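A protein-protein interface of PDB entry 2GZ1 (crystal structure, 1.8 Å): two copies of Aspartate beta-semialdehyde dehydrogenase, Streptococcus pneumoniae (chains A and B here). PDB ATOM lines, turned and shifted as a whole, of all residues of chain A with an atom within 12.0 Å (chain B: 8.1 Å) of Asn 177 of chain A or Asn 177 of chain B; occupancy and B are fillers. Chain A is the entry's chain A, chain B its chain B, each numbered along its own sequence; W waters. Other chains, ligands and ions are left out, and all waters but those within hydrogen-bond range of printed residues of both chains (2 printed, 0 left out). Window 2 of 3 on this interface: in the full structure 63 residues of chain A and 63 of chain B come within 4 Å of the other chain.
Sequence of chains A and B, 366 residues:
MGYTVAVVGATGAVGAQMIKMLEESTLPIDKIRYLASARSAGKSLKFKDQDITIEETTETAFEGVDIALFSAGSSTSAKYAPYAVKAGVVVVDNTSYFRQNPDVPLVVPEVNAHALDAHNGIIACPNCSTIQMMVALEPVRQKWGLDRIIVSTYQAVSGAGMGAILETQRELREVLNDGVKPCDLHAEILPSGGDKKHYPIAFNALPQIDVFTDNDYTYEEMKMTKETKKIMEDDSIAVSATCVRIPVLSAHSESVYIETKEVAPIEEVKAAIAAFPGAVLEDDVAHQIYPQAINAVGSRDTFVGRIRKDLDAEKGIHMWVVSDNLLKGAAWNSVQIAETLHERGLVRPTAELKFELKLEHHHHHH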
ATOM      1  N   LEU A 166      10.031 -14.196  -9.182  1.00  0.00           N
ATOM      2  CA  LEU A 166       9.452 -14.901  -8.041  1.00  0.00           C
ATOM      3  C   LEU A 166       8.524 -16.030  -8.499  1.00  0.00           C
ATOM      4  O   LEU A 166       8.535 -17.112  -7.922  1.00  0.00           O
ATOM      5  CB  LEU A 166       8.716 -13.924  -7.125  1.00  0.00           C
ATOM      6  CG  LEU A 166       9.602 -12.842  -6.481  1.00  0.00           C
ATOM      7  CD1 LEU A 166       8.751 -11.805  -5.744  1.00  0.00           C
ATOM      8  CD2 LEU A 166      10.627 -13.472  -5.549  1.00  0.00           C
ATOM      9  N   GLU A 167       7.741 -15.774  -9.540  1.00  0.00           N
ATOM     10  CA  GLU A 167       6.860 -16.776 -10.129  1.00  0.00           C
ATOM     11  C   GLU A 167       7.653 -17.968 -10.656  1.00  0.00           C
ATOM     12  O   GLU A 167       7.251 -19.105 -10.473  1.00  0.00           O
ATOM     13  CB  GLU A 167       6.072 -16.158 -11.274  1.00  0.00           C
ATOM     14  CG  GLU A 167       5.264 -17.142 -12.099  1.00  0.00           C
ATOM     15  CD  GLU A 167       4.228 -16.439 -12.948  1.00  0.00           C
ATOM     16  OE1 GLU A 167       3.270 -15.903 -12.368  1.00  0.00           O
ATOM     17  OE2 GLU A 167       4.374 -16.412 -14.184  1.00  0.00           O
ATOM     18  N   THR A 168       8.784 -17.693 -11.297  1.00  0.00           N
ATOM     19  CA  THR A 168       9.628 -18.737 -11.856  1.00  0.00           C
ATOM     20  C   THR A 168      10.219 -19.616 -10.762  1.00  0.00           C
ATOM     21  O   THR A 168      10.200 -20.842 -10.867  1.00  0.00           O
ATOM     22  CB  THR A 168      10.744 -18.101 -12.716  1.00  0.00           C
ATOM     23  OG1 THR A 168      10.154 -17.325 -13.766  1.00  0.00           O
ATOM     24  CG2 THR A 168      11.549 -19.155 -13.430  1.00  0.00           C
ATOM     25  N   GLN A 169      10.726 -18.990  -9.704  1.00  0.00           N
ATOM     26  CA  GLN A 169      11.392 -19.720  -8.632  1.00  0.00           C
ATOM     27  C   GLN A 169      10.404 -20.628  -7.904  1.00  0.00           C
ATOM     28  O   GLN A 169      10.721 -21.774  -7.574  1.00  0.00           O
ATOM     29  CB  GLN A 169      12.056 -18.748  -7.649  1.00  0.00           C
ATOM     30  CG  GLN A 169      13.262 -18.031  -8.253  1.00  0.00           C
ATOM     31  CD  GLN A 169      13.800 -16.930  -7.363  1.00  0.00           C
ATOM     32  OE1 GLN A 169      13.042 -16.083  -6.877  1.00  0.00           O
ATOM     33  NE2 GLN A 169      15.104 -16.944  -7.134  1.00  0.00           N
ATOM     34  N   ARG A 170       9.204 -20.117  -7.677  1.00  0.00           N
ATOM     35  CA  ARG A 170       8.204 -20.866  -6.947  1.00  0.00           C
ATOM     36  C   ARG A 170       7.609 -21.981  -7.823  1.00  0.00           C
ATOM     37  O   ARG A 170       7.311 -23.054  -7.329  1.00  0.00           O
ATOM     38  CB  ARG A 170       7.154 -19.917  -6.391  1.00  0.00           C
ATOM     39  CG  ARG A 170       5.933 -19.715  -7.244  1.00  0.00           C
ATOM     40  CD  ARG A 170       4.691 -20.286  -6.627  1.00  0.00           C
ATOM     41  NE  ARG A 170       3.997 -21.106  -7.589  1.00  0.00           N
ATOM     42  CZ  ARG A 170       3.308 -20.644  -8.628  1.00  0.00           C
ATOM     43  NH1 ARG A 170       3.196 -19.352  -8.870  1.00  0.00           N
ATOM     44  NH2 ARG A 170       2.723 -21.505  -9.435  1.00  0.00           N
ATOM     45  N   GLU A 171       7.502 -21.750  -9.130  1.00  0.00           N
ATOM     46  CA  GLU A 171       7.004 -22.793 -10.014  1.00  0.00           C
ATOM     47  C   GLU A 171       7.981 -23.953  -9.998  1.00  0.00           C
ATOM     48  O   GLU A 171       7.578 -25.105  -9.900  1.00  0.00           O
ATOM     49  CB  GLU A 171       6.811 -22.284 -11.442  1.00  0.00           C
ATOM     50  CG  GLU A 171       5.512 -21.513 -11.664  1.00  0.00           C
ATOM     51  CD  GLU A 171       5.422 -20.931 -13.069  1.00  0.00           C
ATOM     52  OE1 GLU A 171       6.219 -21.351 -13.934  1.00  0.00           O
ATOM     53  OE2 GLU A 171       4.564 -20.046 -13.304  1.00  0.00           O
ATOM     54  N   LEU A 172       9.268 -23.637 -10.079  1.00  0.00           N
ATOM     55  CA  LEU A 172      10.305 -24.660 -10.075  1.00  0.00           C
ATOM     56  C   LEU A 172      10.335 -25.429  -8.761  1.00  0.00           C
ATOM     57  O   LEU A 172      10.543 -26.632  -8.754  1.00  0.00           O
ATOM     58  CB  LEU A 172      11.672 -24.037 -10.351  1.00  0.00           C
ATOM     59  CG  LEU A 172      11.864 -23.615 -11.806  1.00  0.00           C
ATOM     60  CD1 LEU A 172      13.060 -22.721 -11.909  1.00  0.00           C
ATOM     61  CD2 LEU A 172      12.014 -24.858 -12.701  1.00  0.00           C
ATOM     62  N   ARG A 173      10.119 -24.734  -7.646  1.00  0.00           N
ATOM     63  CA  ARG A 173      10.093 -25.393  -6.346  1.00  0.00           C
ATOM     64  C   ARG A 173       8.888 -26.314  -6.241  1.00  0.00           C
ATOM     65  O   ARG A 173       8.986 -27.387  -5.670  1.00  0.00           O
ATOM     66  CB  ARG A 173      10.070 -24.371  -5.203  1.00  0.00           C
ATOM     67  CG  ARG A 173      11.415 -23.711  -4.920  1.00  0.00           C
ATOM     68  CD  ARG A 173      11.448 -22.972  -3.584  1.00  0.00           C
ATOM     69  NE  ARG A 173      10.363 -21.997  -3.459  1.00  0.00           N
ATOM     70  CZ  ARG A 173      10.478 -20.689  -3.692  1.00  0.00           C
ATOM     71  NH1 ARG A 173      11.643 -20.159  -4.065  1.00  0.00           N
ATOM     72  NH2 ARG A 173       9.417 -19.902  -3.541  1.00  0.00           N
ATOM     73  N   GLU A 174       7.755 -25.911  -6.805  1.00  0.00           N
ATOM     74  CA  GLU A 174       6.563 -26.757  -6.778  1.00  0.00           C
ATOM     75  C   GLU A 174       6.798 -28.060  -7.563  1.00  0.00           C
ATOM     76  O   GLU A 174       6.391 -29.127  -7.135  1.00  0.00           O
ATOM     77  CB  GLU A 174       5.342 -26.001  -7.311  1.00  0.00           C
ATOM     78  CG  GLU A 174       4.819 -24.942  -6.352  1.00  0.00           C
ATOM     79  CD  GLU A 174       3.463 -24.373  -6.736  1.00  0.00           C
ATOM     80  OE1 GLU A 174       2.606 -24.261  -5.842  1.00  0.00           O
ATOM     81  OE2 GLU A 174       3.240 -24.026  -7.911  1.00  0.00           O
ATOM     82  N   VAL A 175       7.488 -27.970  -8.697  1.00  0.00           N
ATOM     83  CA  VAL A 175       7.777 -29.153  -9.513  1.00  0.00           C
ATOM     84  C   VAL A 175       8.789 -30.053  -8.806  1.00  0.00           C
ATOM     85  O   VAL A 175       8.546 -31.243  -8.618  1.00  0.00           O
ATOM     86  CB  VAL A 175       8.307 -28.756 -10.907  1.00  0.00           C
ATOM     87  CG1 VAL A 175       8.749 -29.993 -11.708  1.00  0.00           C
ATOM     88  CG2 VAL A 175       7.235 -27.984 -11.677  1.00  0.00           C
ATOM     89  N   LEU A 176       9.893 -29.460  -8.367  1.00  0.00           N
ATOM     90  CA  LEU A 176      11.004 -30.207  -7.781  1.00  0.00           C
ATOM     91  C   LEU A 176      10.757 -30.681  -6.343  1.00  0.00           C
ATOM     92  O   LEU A 176      11.212 -31.757  -5.964  1.00  0.00           O
ATOM     93  CB  LEU A 176      12.294 -29.380  -7.860  1.00  0.00           C
ATOM     94  CG  LEU A 176      12.816 -29.122  -9.278  1.00  0.00           C
ATOM     95  CD1 LEU A 176      13.841 -27.998  -9.301  1.00  0.00           C
ATOM     96  CD2 LEU A 176      13.417 -30.389  -9.885  1.00  0.00           C
ATOM     97  N   ASN A 177      10.024 -29.906  -5.551  1.00  0.00           N
ATOM     98  CA  ASN A 177       9.798 -30.243  -4.138  1.00  0.00           C
ATOM     99  C   ASN A 177       8.449 -30.911  -3.856  1.00  0.00           C
ATOM    100  O   ASN A 177       8.370 -31.795  -2.997  1.00  0.00           O
ATOM    101  CB  ASN A 177       9.946 -29.001  -3.243  1.00  0.00           C
ATOM    102  CG  ASN A 177      11.305 -28.330  -3.382  1.00  0.00           C
ATOM    103  OD1 ASN A 177      12.284 -28.952  -3.797  1.00  0.00           O
ATOM    104  ND2 ASN A 177      11.367 -27.046  -3.025  1.00  0.00           N
ATOM    105  N   ASP A 178       7.394 -30.476  -4.550  1.00  0.00           N
ATOM    106  CA  ASP A 178       6.045 -31.037  -4.355  1.00  0.00           C
ATOM    107  C   ASP A 178       5.626 -32.052  -5.420  1.00  0.00           C
ATOM    108  O   ASP A 178       4.586 -32.687  -5.274  1.00  0.00           O
ATOM    109  CB  ASP A 178       4.977 -29.933  -4.309  1.00  0.00           C
ATOM    110  CG  ASP A 178       5.262 -28.889  -3.266  1.00  0.00           C
ATOM    111  OD1 ASP A 178       5.798 -29.248  -2.198  1.00  0.00           O
ATOM    112  OD2 ASP A 178       4.991 -27.680  -3.440  1.00  0.00           O
ATOM    113  N   GLY A 179       6.411 -32.184  -6.487  1.00  0.00           N
ATOM    114  CA  GLY A 179       6.126 -33.135  -7.550  1.00  0.00           C
ATOM    115  C   GLY A 179       5.025 -32.735  -8.516  1.00  0.00           C
ATOM    116  O   GLY A 179       4.460 -33.590  -9.183  1.00  0.00           O
ATOM    117  N   VAL A 180       4.733 -31.443  -8.627  1.00  0.00           N
ATOM    118  CA  VAL A 180       3.688 -30.982  -9.533  1.00  0.00           C
ATOM    119  C   VAL A 180       4.200 -31.132 -10.969  1.00  0.00           C
ATOM    120  O   VAL A 180       5.377 -30.904 -11.237  1.00  0.00           O
ATOM    121  CB  VAL A 180       3.306 -29.507  -9.238  1.00  0.00           C
ATOM    122  CG1 VAL A 180       2.245 -29.011 -10.208  1.00  0.00           C
ATOM    123  CG2 VAL A 180       2.823 -29.356  -7.790  1.00  0.00           C
ATOM    124  N   LYS A 181       3.334 -31.558 -11.882  1.00  0.00           N
ATOM    125  CA  LYS A 181       3.692 -31.619 -13.288  1.00  0.00           C
ATOM    126  C   LYS A 181       3.757 -30.186 -13.797  1.00  0.00           C
ATOM    127  O   LYS A 181       2.889 -29.394 -13.459  1.00  0.00           O
ATOM    128  CB  LYS A 181       2.651 -32.404 -14.082  1.00  0.00           C
ATOM    129  CG  LYS A 181       2.637 -33.890 -13.797  1.00  0.00           C
ATOM    130  CD  LYS A 181       1.641 -34.619 -14.709  1.00  0.00           C
ATOM    131  CE  LYS A 181       1.131 -35.903 -14.079  1.00  0.00           C
ATOM    132  NZ  LYS A 181       0.023 -36.516 -14.876  1.00  0.00           N
ATOM    133  N   PRO A 182       4.781 -29.817 -14.569  1.00  0.00           N
ATOM    134  CA  PRO A 182       4.853 -28.454 -15.100  1.00  0.00           C
ATOM    135  C   PRO A 182       3.563 -27.971 -15.756  1.00  0.00           C
ATOM    136  O   PRO A 182       3.154 -26.839 -15.501  1.00  0.00           O
ATOM    137  CB  PRO A 182       6.004 -28.537 -16.103  1.00  0.00           C
ATOM    138  CG  PRO A 182       6.898 -29.543 -15.496  1.00  0.00           C
ATOM    139  CD  PRO A 182       5.978 -30.597 -14.935  1.00  0.00           C
ATOM    140  N   LEU A 185       0.944 -26.441 -13.418  1.00  0.00           N
ATOM    141  CA  LEU A 185       1.284 -25.243 -12.642  1.00  0.00           C
ATOM    142  C   LEU A 185       0.348 -24.071 -12.930  1.00  0.00           C
ATOM    143  O   LEU A 185      -0.214 -23.956 -14.017  1.00  0.00           O
ATOM    144  CB  LEU A 185       2.715 -24.796 -12.927  1.00  0.00           C
ATOM    145  CG  LEU A 185       3.832 -25.717 -12.443  1.00  0.00           C
ATOM    146  CD1 LEU A 185       5.122 -25.336 -13.140  1.00  0.00           C
ATOM    147  CD2 LEU A 185       3.992 -25.642 -10.926  1.00  0.00           C
ATOM    148  N   ALA A 202       8.436 -22.863 -15.837  1.00  0.00           N
ATOM    149  CA  ALA A 202       9.243 -23.952 -15.300  1.00  0.00           C
ATOM    150  C   ALA A 202       9.340 -25.081 -16.320  1.00  0.00           C
ATOM    151  O   ALA A 202       8.313 -25.583 -16.792  1.00  0.00           O
ATOM    152  CB  ALA A 202       8.649 -24.468 -13.968  1.00  0.00           C
ATOM    153  N   PHE A 203      10.573 -25.426 -16.699  1.00  0.00           N
ATOM    154  CA  PHE A 203      10.855 -26.514 -17.640  1.00  0.00           C
ATOM    155  C   PHE A 203      10.132 -26.326 -18.972  1.00  0.00           C
ATOM    156  O   PHE A 203       9.765 -27.290 -19.636  1.00  0.00           O
ATOM    157  CB  PHE A 203      10.509 -27.874 -17.018  1.00  0.00           C
ATOM    158  CG  PHE A 203      11.302 -28.186 -15.779  1.00  0.00           C
ATOM    159  CD1 PHE A 203      12.678 -28.325 -15.849  1.00  0.00           C
ATOM    160  CD2 PHE A 203      10.688 -28.293 -14.554  1.00  0.00           C
ATOM    161  CE1 PHE A 203      13.431 -28.600 -14.723  1.00  0.00           C
ATOM    162  CE2 PHE A 203      11.437 -28.562 -13.410  1.00  0.00           C
ATOM    163  CZ  PHE A 203      12.815 -28.722 -13.505  1.00  0.00           C
ATOM    164  N   LEU A 249      17.009 -16.946 -14.940  1.00  0.00           N
ATOM    165  CA  LEU A 249      16.610 -15.778 -14.149  1.00  0.00           C
ATOM    166  C   LEU A 249      17.181 -14.494 -14.726  1.00  0.00           C
ATOM    167  O   LEU A 249      16.466 -13.501 -14.850  1.00  0.00           O
ATOM    168  CB  LEU A 249      17.014 -15.902 -12.665  1.00  0.00           C
ATOM    169  CG  LEU A 249      16.379 -17.051 -11.863  1.00  0.00           C
ATOM    170  CD1 LEU A 249      16.606 -16.853 -10.377  1.00  0.00           C
ATOM    171  CD2 LEU A 249      14.892 -17.221 -12.153  1.00  0.00           C
ATOM    172  N   GLN B 169      18.168 -31.671 -12.144  1.00  0.00           N
ATOM    173  CA  GLN B 169      17.264 -31.576 -11.002  1.00  0.00           C
ATOM    174  C   GLN B 169      18.008 -31.215  -9.727  1.00  0.00           C
ATOM    175  O   GLN B 169      17.561 -30.373  -8.958  1.00  0.00           O
ATOM    176  CB  GLN B 169      16.509 -32.878 -10.817  1.00  0.00           C
ATOM    177  CG  GLN B 169      15.547 -33.178 -11.949  1.00  0.00           C
ATOM    178  CD  GLN B 169      14.932 -34.541 -11.814  1.00  0.00           C
ATOM    179  OE1 GLN B 169      15.643 -35.532 -11.649  1.00  0.00           O
ATOM    180  NE2 GLN B 169      13.613 -34.602 -11.864  1.00  0.00           N
ATOM    181  N   ARG B 170      19.148 -31.852  -9.508  1.00  0.00           N
ATOM    182  CA  ARG B 170      19.926 -31.589  -8.324  1.00  0.00           C
ATOM    183  C   ARG B 170      20.561 -30.200  -8.343  1.00  0.00           C
ATOM    184  O   ARG B 170      20.598 -29.543  -7.322  1.00  0.00           O
ATOM    185  CB  ARG B 170      20.927 -32.716  -8.060  1.00  0.00           C
ATOM    186  CG  ARG B 170      22.175 -32.778  -8.904  1.00  0.00           C
ATOM    187  CD  ARG B 170      23.435 -33.040  -8.061  1.00  0.00           C
ATOM    188  NE  ARG B 170      24.196 -31.813  -7.957  1.00  0.00           N
ATOM    189  CZ  ARG B 170      25.129 -31.421  -8.821  1.00  0.00           C
ATOM    190  NH1 ARG B 170      25.741 -30.270  -8.612  1.00  0.00           N
ATOM    191  NH2 ARG B 170      25.455 -32.152  -9.879  1.00  0.00           N
ATOM    192  N   GLU B 171      21.018 -29.745  -9.508  1.00  0.00           N
ATOM    193  CA  GLU B 171      21.556 -28.390  -9.641  1.00  0.00           C
ATOM    194  C   GLU B 171      20.482 -27.367  -9.294  1.00  0.00           C
ATOM    195  O   GLU B 171      20.734 -26.442  -8.527  1.00  0.00           O
ATOM    196  CB  GLU B 171      22.092 -28.133 -11.058  1.00  0.00           C
ATOM    197  CG  GLU B 171      23.468 -28.714 -11.311  1.00  0.00           C
ATOM    198  CD  GLU B 171      23.977 -28.445 -12.720  1.00  0.00           C
ATOM    199  OE1 GLU B 171      23.397 -27.581 -13.413  1.00  0.00           O
ATOM    200  OE2 GLU B 171      24.966 -29.091 -13.132  1.00  0.00           O
ATOM    201  N   LEU B 172      19.281 -27.544  -9.844  1.00  0.00           N
ATOM    202  CA  LEU B 172      18.177 -26.617  -9.579  1.00  0.00           C
ATOM    203  C   LEU B 172      17.764 -26.641  -8.112  1.00  0.00           C
ATOM    204  O   LEU B 172      17.429 -25.604  -7.537  1.00  0.00           O
ATOM    205  CB  LEU B 172      16.971 -26.919 -10.475  1.00  0.00           C
ATOM    206  CG  LEU B 172      17.104 -26.531 -11.950  1.00  0.00           C
ATOM    207  CD1 LEU B 172      16.056 -27.254 -12.795  1.00  0.00           C
ATOM    208  CD2 LEU B 172      16.989 -25.018 -12.139  1.00  0.00           C
ATOM    209  N   ARG B 173      17.804 -27.823  -7.502  1.00  0.00           N
ATOM    210  CA  ARG B 173      17.517 -27.945  -6.076  1.00  0.00           C
ATOM    211  C   ARG B 173      18.580 -27.246  -5.236  1.00  0.00           C
ATOM    212  O   ARG B 173      18.261 -26.619  -4.233  1.00  0.00           O
ATOM    213  CB  ARG B 173      17.391 -29.410  -5.658  1.00  0.00           C
ATOM    214  CG  ARG B 173      16.036 -29.996  -5.974  1.00  0.00           C
ATOM    215  CD  ARG B 173      15.916 -31.483  -5.667  1.00  0.00           C
ATOM    216  NE  ARG B 173      14.608 -31.991  -6.087  1.00  0.00           N
ATOM    217  CZ  ARG B 173      14.407 -33.049  -6.868  1.00  0.00           C
ATOM    218  NH1 ARG B 173      15.417 -33.757  -7.348  1.00  0.00           N
ATOM    219  NH2 ARG B 173      13.168 -33.412  -7.166  1.00  0.00           N
ATOM    220  N   GLU B 174      19.838 -27.341  -5.646  1.00  0.00           N
ATOM    221  CA  GLU B 174      20.919 -26.669  -4.925  1.00  0.00           C
ATOM    222  C   GLU B 174      20.776 -25.146  -5.002  1.00  0.00           C
ATOM    223  O   GLU B 174      21.071 -24.445  -4.041  1.00  0.00           O
ATOM    224  CB  GLU B 174      22.283 -27.109  -5.458  1.00  0.00           C
ATOM    225  CG  GLU B 174      22.683 -28.493  -4.976  1.00  0.00           C
ATOM    226  CD  GLU B 174      23.965 -29.008  -5.599  1.00  0.00           C
ATOM    227  OE1 GLU B 174      24.744 -28.207  -6.153  1.00  0.00           O
ATOM    228  OE2 GLU B 174      24.205 -30.230  -5.514  1.00  0.00           O
ATOM    229  N   VAL B 175      20.310 -24.634  -6.138  1.00  0.00           N
ATOM    230  CA  VAL B 175      20.114 -23.191  -6.288  1.00  0.00           C
ATOM    231  C   VAL B 175      18.903 -22.723  -5.480  1.00  0.00           C
ATOM    232  O   VAL B 175      18.988 -21.772  -4.709  1.00  0.00           O
ATOM    233  CB  VAL B 175      19.913 -22.793  -7.761  1.00  0.00           C
ATOM    234  CG1 VAL B 175      19.514 -21.326  -7.868  1.00  0.00           C
ATOM    235  CG2 VAL B 175      21.176 -23.063  -8.567  1.00  0.00           C
ATOM    236  N   LEU B 176      17.787 -23.421  -5.654  1.00  0.00           N
ATOM    237  CA  LEU B 176      16.492 -22.999  -5.121  1.00  0.00           C
ATOM    238  C   LEU B 176      16.273 -23.297  -3.634  1.00  0.00           C
ATOM    239  O   LEU B 176      15.638 -22.518  -2.939  1.00  0.00           O
ATOM    240  CB  LEU B 176      15.365 -23.656  -5.924  1.00  0.00           C
ATOM    241  CG  LEU B 176      15.188 -23.105  -7.341  1.00  0.00           C
ATOM    242  CD1 LEU B 176      14.374 -24.062  -8.165  1.00  0.00           C
ATOM    243  CD2 LEU B 176      14.513 -21.744  -7.295  1.00  0.00           C
ATOM    244  N   ASN B 177      16.764 -24.435  -3.161  1.00  0.00           N
ATOM    245  CA  ASN B 177      16.580 -24.822  -1.763  1.00  0.00           C
ATOM    246  C   ASN B 177      17.776 -24.448  -0.893  1.00  0.00           C
ATOM    247  O   ASN B 177      17.597 -24.036   0.251  1.00  0.00           O
ATOM    248  CB  ASN B 177      16.291 -26.326  -1.635  1.00  0.00           C
ATOM    249  CG  ASN B 177      15.083 -26.765  -2.453  1.00  0.00           C
ATOM    250  OD1 ASN B 177      14.157 -25.987  -2.690  1.00  0.00           O
ATOM    251  ND2 ASN B 177      15.086 -28.022  -2.878  1.00  0.00           N
ATOM    252  N   ASP B 178      18.985 -24.601  -1.433  1.00  0.00           N
ATOM    253  CA  ASP B 178      20.215 -24.377  -0.668  1.00  0.00           C
ATOM    254  C   ASP B 178      20.863 -23.004  -0.903  1.00  0.00           C
ATOM    255  O   ASP B 178      21.842 -22.664  -0.247  1.00  0.00           O
ATOM    256  CB  ASP B 178      21.235 -25.482  -0.978  1.00  0.00           C
ATOM    257  CG  ASP B 178      20.698 -26.882  -0.698  1.00  0.00           C
ATOM    258  OD1 ASP B 178      19.803 -27.037   0.157  1.00  0.00           O
ATOM    259  OD2 ASP B 178      21.126 -27.892  -1.291  1.00  0.00           O
ATOM    260  N   GLY B 179      20.328 -22.223  -1.838  1.00  0.00           N
ATOM    261  CA  GLY B 179      20.826 -20.879  -2.096  1.00  0.00           C
ATOM    262  C   GLY B 179      22.189 -20.795  -2.772  1.00  0.00           C
ATOM    263  O   GLY B 179      22.878 -19.787  -2.654  1.00  0.00           O
ATOM    264  N   VAL B 180      22.573 -21.847  -3.488  1.00  0.00           N
ATOM    265  CA  VAL B 180      23.826 -21.879  -4.236  1.00  0.00           C
ATOM    266  C   VAL B 180      23.691 -21.004  -5.485  1.00  0.00           C
ATOM    267  O   VAL B 180      22.660 -21.033  -6.140  1.00  0.00           O
ATOM    268  CB  VAL B 180      24.178 -23.337  -4.647  1.00  0.00           C
ATOM    269  CG1 VAL B 180      25.428 -23.390  -5.528  1.00  0.00           C
ATOM    270  CG2 VAL B 180      24.345 -24.223  -3.410  1.00  0.00           C
HETATM  271  O   HOH W   1      14.380 -20.480  -3.790  1.00  0.00           O
HETATM  272  O   HOH W   2      13.499 -31.509  -3.655  1.00  0.00           O
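NH2 of Arg 173 of chain B is in hydrogen-bond range of O of Leu 176 of chain A, at 2.8 Å.
The side-chain amide oxygen (OD1) of Asn 177 of chain B sits at hydrogen-bond distance from the side-chain amide nitrogen (ND2) of Asn 177 of chain A, 3.0 Å away.
Among the printed residues, pairs that only touch across the chains: Gln 169 of chain A with Leu 176 of chain B, Leu 172 of chain A with Leu 176 of chain B, Leu 176 of chain A with Leu 172 of chain B and Phe 203 of chain A with Leu 172 of chain B.
Printed residues of chain B within 4 Å of Leu 172 of chain A: Leu 176 (3.5 Å).
Of the printed residues of chain B, Leu 176 of chain A touches Leu 172 (3.5 Å) and Arg 173 (2.8 Å).
Asn 177 of chain A touches just one residue of chain B: Asn 177 (3.0 Å).
Of the printed residues of chain A, Leu 172 of chain B touches Leu 176 (3.5 Å) and Phe 203 (3.5 Å).
Arg 173 of chain B touches just one residue of chain A: Leu 176.
Leu 176 of chain B touches just these residues of chain A: Gln 169 (3.8 Å) and Leu 172 (3.5 Å).
Asn 177 of chain B touches just one residue of chain A: Asn 177 (3.0 Å).
Val 180 of chain B touches none of the printed residues of chain A.
The nearest residue of chain B that does not touch Asn 177 of chain A is Arg 173 of chain B (4.5 Å).
The nearest residue of chain A that does not touch Asn 177 of chain B is Arg 173 of chain A (4.2 Å).
The nearest printed residue of chain B that does not touch Phe 203 of chain A is Gln 169 of chain B (5.5 Å).
Of the 12 printed residues of chain B, 4 touch a printed residue of chain A.
Among the printed residues, 6 pairs touch across the chains.
Among the printed residues, no Asp or Glu carboxylate lies within 4 Å of a Lys or Arg side-chain nitrogen of the other chain.
Gln 169 of chain A touches Leu 176 of chain B, but with the chains exchanged Leu 176 of chain A does not touch Gln 169 of chain B (4.1 Å).
Leu 172 of chain A touches Leu 176 of chain B, and with the chains exchanged Leu 176 of chain A touches Leu 172 of chain B.
Leu 176 of chain A touches Arg 173 of chain B, but with the chains exchanged Arg 173 of chain A does not touch Leu 176 of chain B (4.1 Å).
Asn 177 of chain A touches its own counterpart, Asn 177 of chain B.
Water W1 lies within hydrogen-bond range of O of Leu 176 of chain B (2.5 Å) and NH1 of Arg 173 of chain A (2.8 Å).
Water W2 lies within hydrogen-bond range of the guanidinium group of Arg 173 of chain B (2.7 Å), the side-chain amide oxygen of Asn 177 of chain A (2.8 Å) and the backbone carbonyl oxygen of Leu 176 of chain A (3.3 Å).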
